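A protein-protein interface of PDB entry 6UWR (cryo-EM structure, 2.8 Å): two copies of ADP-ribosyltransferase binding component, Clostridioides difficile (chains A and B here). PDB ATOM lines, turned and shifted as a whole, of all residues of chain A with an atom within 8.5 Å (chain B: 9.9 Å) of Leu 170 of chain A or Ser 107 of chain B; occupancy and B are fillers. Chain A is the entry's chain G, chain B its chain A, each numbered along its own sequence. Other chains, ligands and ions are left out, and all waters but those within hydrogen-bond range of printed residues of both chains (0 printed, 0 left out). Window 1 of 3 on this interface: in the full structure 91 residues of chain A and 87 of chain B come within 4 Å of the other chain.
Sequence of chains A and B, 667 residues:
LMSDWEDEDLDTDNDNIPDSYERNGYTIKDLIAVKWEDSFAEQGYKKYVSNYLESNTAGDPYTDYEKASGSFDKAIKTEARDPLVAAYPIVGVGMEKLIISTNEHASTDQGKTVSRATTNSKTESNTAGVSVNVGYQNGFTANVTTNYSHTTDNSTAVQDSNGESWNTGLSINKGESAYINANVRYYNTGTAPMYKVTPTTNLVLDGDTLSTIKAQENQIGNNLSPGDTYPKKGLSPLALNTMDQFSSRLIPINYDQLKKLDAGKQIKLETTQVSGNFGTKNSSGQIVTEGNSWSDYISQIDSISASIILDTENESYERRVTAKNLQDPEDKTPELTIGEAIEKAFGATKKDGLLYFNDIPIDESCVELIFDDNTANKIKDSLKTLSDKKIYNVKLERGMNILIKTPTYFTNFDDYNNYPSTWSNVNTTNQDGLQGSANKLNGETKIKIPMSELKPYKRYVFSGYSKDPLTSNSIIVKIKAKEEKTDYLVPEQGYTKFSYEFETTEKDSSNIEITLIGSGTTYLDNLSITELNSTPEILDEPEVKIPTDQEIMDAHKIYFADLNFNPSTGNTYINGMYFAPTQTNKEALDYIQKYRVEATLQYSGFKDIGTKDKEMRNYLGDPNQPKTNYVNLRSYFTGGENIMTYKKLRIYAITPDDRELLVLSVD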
ATOM      1  N   THR A 102     -30.887   4.859 -33.774  1.00  0.00           N
ATOM      2  CA  THR A 102     -29.761   5.722 -33.457  1.00  0.00           C
ATOM      3  C   THR A 102     -28.825   5.039 -32.469  1.00  0.00           C
ATOM      4  O   THR A 102     -29.263   4.454 -31.482  1.00  0.00           O
ATOM      5  CB  THR A 102     -30.256   7.048 -32.889  1.00  0.00           C
ATOM      6  OG1 THR A 102     -31.663   7.158 -33.113  1.00  0.00           O
ATOM      7  CG2 THR A 102     -29.573   8.200 -33.567  1.00  0.00           C
ATOM      8  N   ASN A 103     -27.528   5.114 -32.749  1.00  0.00           N
ATOM      9  CA  ASN A 103     -26.515   4.421 -31.959  1.00  0.00           C
ATOM     10  C   ASN A 103     -25.908   5.410 -30.969  1.00  0.00           C
ATOM     11  O   ASN A 103     -24.785   5.885 -31.125  1.00  0.00           O
ATOM     12  CB  ASN A 103     -25.461   3.807 -32.876  1.00  0.00           C
ATOM     13  CG  ASN A 103     -24.560   2.836 -32.158  1.00  0.00           C
ATOM     14  OD1 ASN A 103     -24.985   2.148 -31.235  1.00  0.00           O
ATOM     15  ND2 ASN A 103     -23.304   2.774 -32.578  1.00  0.00           N
ATOM     16  N   GLU A 104     -26.672   5.713 -29.928  1.00  0.00           N
ATOM     17  CA  GLU A 104     -26.264   6.638 -28.884  1.00  0.00           C
ATOM     18  C   GLU A 104     -26.173   5.919 -27.551  1.00  0.00           C
ATOM     19  O   GLU A 104     -26.810   4.890 -27.335  1.00  0.00           O
ATOM     20  CB  GLU A 104     -27.246   7.797 -28.748  1.00  0.00           C
ATOM     21  CG  GLU A 104     -27.291   8.713 -29.926  1.00  0.00           C
ATOM     22  CD  GLU A 104     -28.398   9.724 -29.807  1.00  0.00           C
ATOM     23  OE1 GLU A 104     -29.415   9.408 -29.160  1.00  0.00           O
ATOM     24  OE2 GLU A 104     -28.254  10.835 -30.358  1.00  0.00           O
ATOM     25  N   HIS A 105     -25.383   6.493 -26.650  1.00  0.00           N
ATOM     26  CA  HIS A 105     -25.260   6.025 -25.276  1.00  0.00           C
ATOM     27  C   HIS A 105     -25.616   7.173 -24.349  1.00  0.00           C
ATOM     28  O   HIS A 105     -24.957   8.214 -24.368  1.00  0.00           O
ATOM     29  CB  HIS A 105     -23.849   5.522 -24.996  1.00  0.00           C
ATOM     30  CG  HIS A 105     -23.474   4.315 -25.790  1.00  0.00           C
ATOM     31  ND1 HIS A 105     -23.697   3.033 -25.343  1.00  0.00           N
ATOM     32  CD2 HIS A 105     -22.900   4.194 -27.009  1.00  0.00           C
ATOM     33  CE1 HIS A 105     -23.273   2.174 -26.251  1.00  0.00           C
ATOM     34  NE2 HIS A 105     -22.785   2.853 -27.272  1.00  0.00           N
ATOM     35  N   ALA A 106     -26.654   6.986 -23.542  1.00  0.00           N
ATOM     36  CA  ALA A 106     -27.163   8.024 -22.660  1.00  0.00           C
ATOM     37  C   ALA A 106     -26.951   7.611 -21.214  1.00  0.00           C
ATOM     38  O   ALA A 106     -27.209   6.463 -20.850  1.00  0.00           O
ATOM     39  CB  ALA A 106     -28.642   8.285 -22.926  1.00  0.00           C
ATOM     40  N   SER A 107     -26.488   8.547 -20.392  1.00  0.00           N
ATOM     41  CA  SER A 107     -26.197   8.291 -18.993  1.00  0.00           C
ATOM     42  C   SER A 107     -27.011   9.215 -18.100  1.00  0.00           C
ATOM     43  O   SER A 107     -27.490  10.265 -18.528  1.00  0.00           O
ATOM     44  CB  SER A 107     -24.713   8.480 -18.703  1.00  0.00           C
ATOM     45  OG  SER A 107     -23.932   7.795 -19.657  1.00  0.00           O
ATOM     46  N   THR A 108     -27.165   8.803 -16.842  1.00  0.00           N
ATOM     47  CA  THR A 108     -27.825   9.616 -15.820  1.00  0.00           C
ATOM     48  C   THR A 108     -27.208   9.237 -14.481  1.00  0.00           C
ATOM     49  O   THR A 108     -27.592   8.228 -13.889  1.00  0.00           O
ATOM     50  CB  THR A 108     -29.333   9.408 -15.796  1.00  0.00           C
ATOM     51  OG1 THR A 108     -29.648   8.062 -16.164  1.00  0.00           O
ATOM     52  CG2 THR A 108     -30.043  10.375 -16.713  1.00  0.00           C
ATOM     53  N   ASN A 167     -25.906  14.362 -13.187  1.00  0.00           N
ATOM     54  CA  ASN A 167     -25.206  14.433 -14.461  1.00  0.00           C
ATOM     55  C   ASN A 167     -25.969  13.655 -15.516  1.00  0.00           C
ATOM     56  O   ASN A 167     -26.449  12.553 -15.253  1.00  0.00           O
ATOM     57  CB  ASN A 167     -23.793  13.875 -14.360  1.00  0.00           C
ATOM     58  CG  ASN A 167     -22.898  14.719 -13.504  1.00  0.00           C
ATOM     59  OD1 ASN A 167     -22.178  15.577 -14.003  1.00  0.00           O
ATOM     60  ND2 ASN A 167     -22.933  14.484 -12.200  1.00  0.00           N
ATOM     61  N   THR A 168     -26.075  14.230 -16.708  1.00  0.00           N
ATOM     62  CA  THR A 168     -26.601  13.538 -17.874  1.00  0.00           C
ATOM     63  C   THR A 168     -25.558  13.590 -18.974  1.00  0.00           C
ATOM     64  O   THR A 168     -24.959  14.637 -19.216  1.00  0.00           O
ATOM     65  CB  THR A 168     -27.896  14.164 -18.384  1.00  0.00           C
ATOM     66  OG1 THR A 168     -27.789  15.588 -18.352  1.00  0.00           O
ATOM     67  CG2 THR A 168     -29.059  13.748 -17.515  1.00  0.00           C
ATOM     68  N   GLY A 169     -25.339  12.458 -19.639  1.00  0.00           N
ATOM     69  CA  GLY A 169     -24.353  12.375 -20.689  1.00  0.00           C
ATOM     70  C   GLY A 169     -24.973  11.896 -21.989  1.00  0.00           C
ATOM     71  O   GLY A 169     -26.121  11.462 -22.033  1.00  0.00           O
ATOM     72  N   LEU A 170     -24.184  11.999 -23.052  1.00  0.00           N
ATOM     73  CA  LEU A 170     -24.592  11.504 -24.362  1.00  0.00           C
ATOM     74  C   LEU A 170     -23.351  11.368 -25.223  1.00  0.00           C
ATOM     75  O   LEU A 170     -22.722  12.374 -25.547  1.00  0.00           O
ATOM     76  CB  LEU A 170     -25.591  12.444 -25.010  1.00  0.00           C
ATOM     77  CG  LEU A 170     -26.200  11.976 -26.326  1.00  0.00           C
ATOM     78  CD1 LEU A 170     -27.148  10.829 -26.082  1.00  0.00           C
ATOM     79  CD2 LEU A 170     -26.919  13.117 -27.001  1.00  0.00           C
ATOM     80  N   SER A 171     -23.004  10.141 -25.592  1.00  0.00           N
ATOM     81  CA  SER A 171     -21.902   9.878 -26.503  1.00  0.00           C
ATOM     82  C   SER A 171     -22.447   9.502 -27.870  1.00  0.00           C
ATOM     83  O   SER A 171     -23.522   8.909 -27.979  1.00  0.00           O
ATOM     84  CB  SER A 171     -21.001   8.764 -25.982  1.00  0.00           C
ATOM     85  OG  SER A 171     -21.222   8.534 -24.608  1.00  0.00           O
ATOM     86  N   ILE A 172     -21.696   9.842 -28.910  1.00  0.00           N
ATOM     87  CA  ILE A 172     -22.124   9.662 -30.290  1.00  0.00           C
ATOM     88  C   ILE A 172     -20.929   9.198 -31.107  1.00  0.00           C
ATOM     89  O   ILE A 172     -19.852   9.794 -31.030  1.00  0.00           O
ATOM     90  CB  ILE A 172     -22.704  10.966 -30.870  1.00  0.00           C
ATOM     91  CG1 ILE A 172     -24.095  11.231 -30.300  1.00  0.00           C
ATOM     92  CG2 ILE A 172     -22.755  10.914 -32.376  1.00  0.00           C
ATOM     93  CD1 ILE A 172     -24.634  12.602 -30.618  1.00  0.00           C
ATOM     94  N   ASN A 173     -21.113   8.132 -31.873  1.00  0.00           N
ATOM     95  CA  ASN A 173     -20.125   7.686 -32.841  1.00  0.00           C
ATOM     96  C   ASN A 173     -20.429   8.325 -34.186  1.00  0.00           C
ATOM     97  O   ASN A 173     -21.551   8.222 -34.684  1.00  0.00           O
ATOM     98  CB  ASN A 173     -20.155   6.166 -32.961  1.00  0.00           C
ATOM     99  CG  ASN A 173     -18.854   5.589 -33.452  1.00  0.00           C
ATOM    100  OD1 ASN A 173     -18.557   4.426 -33.208  1.00  0.00           O
ATOM    101  ND2 ASN A 173     -18.071   6.394 -34.149  1.00  0.00           N
ATOM    102  N   LYS A 174     -19.442   8.989 -34.768  1.00  0.00           N
ATOM    103  CA  LYS A 174     -19.647   9.627 -36.057  1.00  0.00           C
ATOM    104  C   LYS A 174     -19.442   8.680 -37.226  1.00  0.00           C
ATOM    105  O   LYS A 174     -19.762   9.045 -38.359  1.00  0.00           O
ATOM    106  CB  LYS A 174     -18.719  10.827 -36.208  1.00  0.00           C
ATOM    107  CG  LYS A 174     -18.763  11.777 -35.046  1.00  0.00           C
ATOM    108  CD  LYS A 174     -19.994  12.629 -35.094  1.00  0.00           C
ATOM    109  CE  LYS A 174     -19.761  13.941 -34.398  1.00  0.00           C
ATOM    110  NZ  LYS A 174     -18.609  14.664 -34.983  1.00  0.00           N
ATOM    111  N   GLU B 104     -14.879   9.008 -35.040  1.00  0.00           N
ATOM    112  CA  GLU B 104     -14.747   9.836 -33.853  1.00  0.00           C
ATOM    113  C   GLU B 104     -15.838   9.500 -32.853  1.00  0.00           C
ATOM    114  O   GLU B 104     -16.898   8.991 -33.212  1.00  0.00           O
ATOM    115  CB  GLU B 104     -14.835  11.320 -34.192  1.00  0.00           C
ATOM    116  CG  GLU B 104     -13.704  11.837 -35.017  1.00  0.00           C
ATOM    117  CD  GLU B 104     -13.938  13.253 -35.466  1.00  0.00           C
ATOM    118  OE1 GLU B 104     -15.115  13.631 -35.625  1.00  0.00           O
ATOM    119  OE2 GLU B 104     -12.950  13.990 -35.660  1.00  0.00           O
ATOM    120  N   HIS B 105     -15.565   9.813 -31.591  1.00  0.00           N
ATOM    121  CA  HIS B 105     -16.529   9.681 -30.507  1.00  0.00           C
ATOM    122  C   HIS B 105     -16.692  11.040 -29.848  1.00  0.00           C
ATOM    123  O   HIS B 105     -15.726  11.593 -29.320  1.00  0.00           O
ATOM    124  CB  HIS B 105     -16.071   8.641 -29.492  1.00  0.00           C
ATOM    125  CG  HIS B 105     -16.005   7.256 -30.044  1.00  0.00           C
ATOM    126  ND1 HIS B 105     -17.072   6.387 -30.002  1.00  0.00           N
ATOM    127  CD2 HIS B 105     -15.001   6.589 -30.661  1.00  0.00           C
ATOM    128  CE1 HIS B 105     -16.728   5.244 -30.566  1.00  0.00           C
ATOM    129  NE2 HIS B 105     -15.477   5.341 -30.974  1.00  0.00           N
ATOM    130  N   ALA B 106     -17.906  11.574 -29.879  1.00  0.00           N
ATOM    131  CA  ALA B 106     -18.196  12.903 -29.362  1.00  0.00           C
ATOM    132  C   ALA B 106     -19.117  12.793 -28.160  1.00  0.00           C
ATOM    133  O   ALA B 106     -20.087  12.036 -28.188  1.00  0.00           O
ATOM    134  CB  ALA B 106     -18.832  13.776 -30.440  1.00  0.00           C
ATOM    135  N   SER B 107     -18.817  13.551 -27.113  1.00  0.00           N
ATOM    136  CA  SER B 107     -19.578  13.523 -25.876  1.00  0.00           C
ATOM    137  C   SER B 107     -20.125  14.906 -25.555  1.00  0.00           C
ATOM    138  O   SER B 107     -19.628  15.921 -26.042  1.00  0.00           O
ATOM    139  CB  SER B 107     -18.719  13.032 -24.718  1.00  0.00           C
ATOM    140  OG  SER B 107     -18.034  11.852 -25.076  1.00  0.00           O
ATOM    141  N   THR B 108     -21.166  14.929 -24.722  1.00  0.00           N
ATOM    142  CA  THR B 108     -21.746  16.174 -24.220  1.00  0.00           C
ATOM    143  C   THR B 108     -22.334  15.870 -22.849  1.00  0.00           C
ATOM    144  O   THR B 108     -23.444  15.346 -22.756  1.00  0.00           O
ATOM    145  CB  THR B 108     -22.813  16.735 -25.151  1.00  0.00           C
ATOM    146  OG1 THR B 108     -23.499  15.665 -25.810  1.00  0.00           O
ATOM    147  CG2 THR B 108     -22.222  17.678 -26.171  1.00  0.00           C
ATOM    148  N   ASP B 109     -21.606  16.222 -21.802  1.00  0.00           N
ATOM    149  CA  ASP B 109     -22.064  16.031 -20.438  1.00  0.00           C
ATOM    150  C   ASP B 109     -22.514  17.366 -19.869  1.00  0.00           C
ATOM    151  O   ASP B 109     -21.933  18.404 -20.181  1.00  0.00           O
ATOM    152  CB  ASP B 109     -20.945  15.453 -19.580  1.00  0.00           C
ATOM    153  CG  ASP B 109     -20.384  14.171 -20.151  1.00  0.00           C
ATOM    154  OD1 ASP B 109     -19.144  14.016 -20.162  1.00  0.00           O
ATOM    155  OD2 ASP B 109     -21.174  13.326 -20.620  1.00  0.00           O
ATOM    156  N   GLN B 110     -23.555  17.343 -19.046  1.00  0.00           N
ATOM    157  CA  GLN B 110     -23.948  18.523 -18.292  1.00  0.00           C
ATOM    158  C   GLN B 110     -24.383  18.111 -16.898  1.00  0.00           C
ATOM    159  O   GLN B 110     -25.095  17.121 -16.727  1.00  0.00           O
ATOM    160  CB  GLN B 110     -25.059  19.306 -18.983  1.00  0.00           C
ATOM    161  CG  GLN B 110     -26.339  18.556 -19.185  1.00  0.00           C
ATOM    162  CD  GLN B 110     -27.321  19.318 -20.047  1.00  0.00           C
ATOM    163  OE1 GLN B 110     -27.192  20.526 -20.231  1.00  0.00           O
ATOM    164  NE2 GLN B 110     -28.309  18.615 -20.583  1.00  0.00           N
ATOM    165  N   TRP B 166     -20.790  22.080 -18.076  1.00  0.00           N
ATOM    166  CA  TRP B 166     -20.999  21.627 -19.443  1.00  0.00           C
ATOM    167  C   TRP B 166     -19.664  21.126 -19.955  1.00  0.00           C
ATOM    168  O   TRP B 166     -18.699  21.888 -19.977  1.00  0.00           O
ATOM    169  CB  TRP B 166     -21.518  22.756 -20.329  1.00  0.00           C
ATOM    170  CG  TRP B 166     -22.821  23.328 -19.898  1.00  0.00           C
ATOM    171  CD1 TRP B 166     -24.058  22.918 -20.280  1.00  0.00           C
ATOM    172  CD2 TRP B 166     -23.022  24.428 -19.007  1.00  0.00           C
ATOM    173  NE1 TRP B 166     -25.020  23.684 -19.677  1.00  0.00           N
ATOM    174  CE2 TRP B 166     -24.408  24.619 -18.889  1.00  0.00           C
ATOM    175  CE3 TRP B 166     -22.164  25.265 -18.293  1.00  0.00           C
ATOM    176  CZ2 TRP B 166     -24.954  25.612 -18.091  1.00  0.00           C
ATOM    177  CZ3 TRP B 166     -22.708  26.245 -17.501  1.00  0.00           C
ATOM    178  CH2 TRP B 166     -24.088  26.413 -17.406  1.00  0.00           C
ATOM    179  N   ASN B 167     -19.598  19.864 -20.361  1.00  0.00           N
ATOM    180  CA  ASN B 167     -18.384  19.287 -20.916  1.00  0.00           C
ATOM    181  C   ASN B 167     -18.655  18.752 -22.309  1.00  0.00           C
ATOM    182  O   ASN B 167     -19.684  18.117 -22.544  1.00  0.00           O
ATOM    183  CB  ASN B 167     -17.849  18.156 -20.048  1.00  0.00           C
ATOM    184  CG  ASN B 167     -17.345  18.636 -18.720  1.00  0.00           C
ATOM    185  OD1 ASN B 167     -16.157  18.892 -18.554  1.00  0.00           O
ATOM    186  ND2 ASN B 167     -18.245  18.760 -17.757  1.00  0.00           N
ATOM    187  N   THR B 168     -17.731  19.007 -23.228  1.00  0.00           N
ATOM    188  CA  THR B 168     -17.744  18.404 -24.551  1.00  0.00           C
ATOM    189  C   THR B 168     -16.427  17.684 -24.763  1.00  0.00           C
ATOM    190  O   THR B 168     -15.365  18.220 -24.447  1.00  0.00           O
ATOM    191  CB  THR B 168     -17.934  19.439 -25.657  1.00  0.00           C
ATOM    192  OG1 THR B 168     -17.142  20.595 -25.376  1.00  0.00           O
ATOM    193  CG2 THR B 168     -19.381  19.856 -25.746  1.00  0.00           C
ATOM    194  N   GLY B 169     -16.494  16.468 -25.301  1.00  0.00           N
ATOM    195  CA  GLY B 169     -15.311  15.674 -25.528  1.00  0.00           C
ATOM    196  C   GLY B 169     -15.195  15.265 -26.984  1.00  0.00           C
ATOM    197  O   GLY B 169     -16.115  15.444 -27.779  1.00  0.00           O
ATOM    198  N   LEU B 170     -14.031  14.719 -27.317  1.00  0.00           N
ATOM    199  CA  LEU B 170     -13.785  14.191 -28.654  1.00  0.00           C
ATOM    200  C   LEU B 170     -12.581  13.274 -28.585  1.00  0.00           C
ATOM    201  O   LEU B 170     -11.473  13.741 -28.320  1.00  0.00           O
ATOM    202  CB  LEU B 170     -13.544  15.315 -29.645  1.00  0.00           C
ATOM    203  CG  LEU B 170     -13.407  14.904 -31.107  1.00  0.00           C
ATOM    204  CD1 LEU B 170     -14.740  14.455 -31.649  1.00  0.00           C
ATOM    205  CD2 LEU B 170     -12.871  16.056 -31.920  1.00  0.00           C
ATOM    206  N   SER B 171     -12.788  11.985 -28.825  1.00  0.00           N
ATOM    207  CA  SER B 171     -11.708  11.015 -28.897  1.00  0.00           C
ATOM    208  C   SER B 171     -11.452  10.640 -30.347  1.00  0.00           C
ATOM    209  O   SER B 171     -12.371  10.636 -31.167  1.00  0.00           O
ATOM    210  CB  SER B 171     -12.026   9.763 -28.088  1.00  0.00           C
ATOM    211  OG  SER B 171     -13.082  10.000 -27.183  1.00  0.00           O
ATOM    212  N   ILE B 172     -10.202  10.319 -30.654  1.00  0.00           N
ATOM    213  CA  ILE B 172      -9.762  10.050 -32.016  1.00  0.00           C
ATOM    214  C   ILE B 172      -8.782   8.888 -31.983  1.00  0.00           C
ATOM    215  O   ILE B 172      -7.842   8.888 -31.186  1.00  0.00           O
ATOM    216  CB  ILE B 172      -9.110  11.292 -32.649  1.00  0.00           C
ATOM    217  CG1 ILE B 172     -10.174  12.324 -33.019  1.00  0.00           C
ATOM    218  CG2 ILE B 172      -8.296  10.920 -33.862  1.00  0.00           C
ATOM    219  CD1 ILE B 172      -9.611  13.666 -33.414  1.00  0.00           C
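Of chain B, only Ala 106, Ser 107 and Thr 108 come within 4 Å of Leu 170 of chain A.
Ser 107 of chain B touches just one residue of chain A: Leu 170.
Gly 169 of chain A touches just these residues of chain B: Thr 108 and Asp 109.
Ala 106 of chain B touches three residues of chain A.
Of chain A, only Thr 168, Gly 169 and Leu 170 come within 4 Å of Thr 108 of chain B.
Printed residues of chain B within 4 Å of Lys 174 of chain A: Glu 104 (3.0 Å).
Of the printed residues of chain A, Glu 104 of chain B touches Ile 172 (3.8 Å), Asn 173 (3.0 Å) and Lys 174 (3.0 Å).
Printed residues of chain B within 4 Å of Thr 168 of chain A: Thr 108, Asp 109 and Gln 110.
Of the printed residues of chain A, Asp 109 of chain B touches Thr 168 (3.4 Å) and Gly 169 (3.3 Å).
Thr 108 of chain A touches none of the printed residues of chain B.
The nearest residue of chain A that does not touch Ser 107 of chain B is Ser 171 of chain A (4.4 Å).
The nearest printed residue of chain A that does not touch Asp 109 of chain B is Leu 170 of chain A (4.1 Å).
Leu 170 of chain A touches Ala 106 of chain B, but with the chains exchanged Ala 106 of chain A does not touch Leu 170 of chain B (15.3 Å).
Leu 170 of chain A touches Ser 107 of chain B, but with the chains exchanged Ser 107 of chain A does not touch Leu 170 of chain B (14.3 Å).
Ile 172 of chain A touches His 105 of chain B, but with the chains exchanged His 105 of chain A does not touch Ile 172 of chain B (14.6 Å).
Ile 172 of chain A touches Ala 106 of chain B, but with the chains exchanged Ala 106 of chain A does not touch Ile 172 of chain B (18.2 Å).
11 positions are printed for both chains.
Of the 16 pairs that touch across the chains among the printed residues, none has its exchanged pair printed and touching as well.
Of the 14 printed residues of chain B, 7 touch a printed residue of chain A.
Hydrophobic or aromatic side chains of chain B that line the printed part of chain A: His 105.
Along chain B the printed residues that touch a printed residue of chain A span positions 104 to 110.
Printed residues of chain A that touch a printed residue of chain B: Asn 167, Thr 168, Gly 169, Leu 170, Ser 171, Ile 172, Asn 173 and Lys 174.
Hydrophobic or aromatic side chains of chain A within 4 Å of the printed part of chain B: Leu 170 and Ile 172.
Among the printed residues, Asp or Glu carboxylates within 4 Å of a Lys or Arg side-chain nitrogen of the other chain: Lys 174 of chain A with Glu 104 of chain B (3.7 Å).
The backbone NH (N) of Ser 171 of chain A is in hydrogen-bond range of the backbone carbonyl oxygen (O) of His 105 of chain A (3.0 Å).
N of Asn 167 of chain B sits at hydrogen-bond distance from O of Asp 109 of chain B (2.8 Å).
O of Ser 107 of chain B is in hydrogen-bond range of N of Gly 169 of chain B (3.3 Å).
The backbone NH of Gly 169 of chain A is in hydrogen-bond range of the backbone carbonyl oxygen of Ser 107 of chain A, 3.3 Å away.
The backbone carbonyl oxygen (O) of His 105 of chain B lies within hydrogen-bond range of the backbone NH (N) of Ser 171 of chain B, at 3.0 Å.
Asn 167 of chain A touches Gln 110 of chain B.
Thr 108 of chain B touches Thr 168 of chain A.
CA of Gly 169 of chain A touches O of Thr 108 of chain B (3.7 Å).
OD2 of Asp 109 of chain B touches CA of Gly 169 of chain A, at 3.3 Å.
O of Ala 106 of chain B touches O of Leu 170 of chain A, 3.7 Å away.
Leu 170 of chain A touches Ser 107 of chain B.
O of Ala 106 of chain B touches CA of Ser 171 of chain A (3.3 Å).
Glu 104 of chain B touches Ile 172 of chain A (O to O, 3.8 Å).
Ile 172 of chain A touches His 105 of chain B (O to CA, 3.4 Å).
Asn 173 of chain A touches His 105 of chain B (OD1 to CE1, 3.3 Å).
O of Gln 110 of chain B sits at hydrogen-bond distance from N of Thr 168 of chain A (3.1 Å).
ND2 of Asn 173 of chain A is in hydrogen-bond range of O of Glu 104 of chain B, 3.0 Å away.
NZ of Lys 174 of chain A is in salt-bridge range of OE1 of Glu 104 of chain B.
The backbone carbonyl oxygen of Ala 106 of chain B sits at hydrogen-bond distance from the backbone NH of Ile 172 of chain A, at 2.8 Å.
O of Leu 170 of chain A lies within hydrogen-bond range of N of Thr 108 of chain B (3.1 Å).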
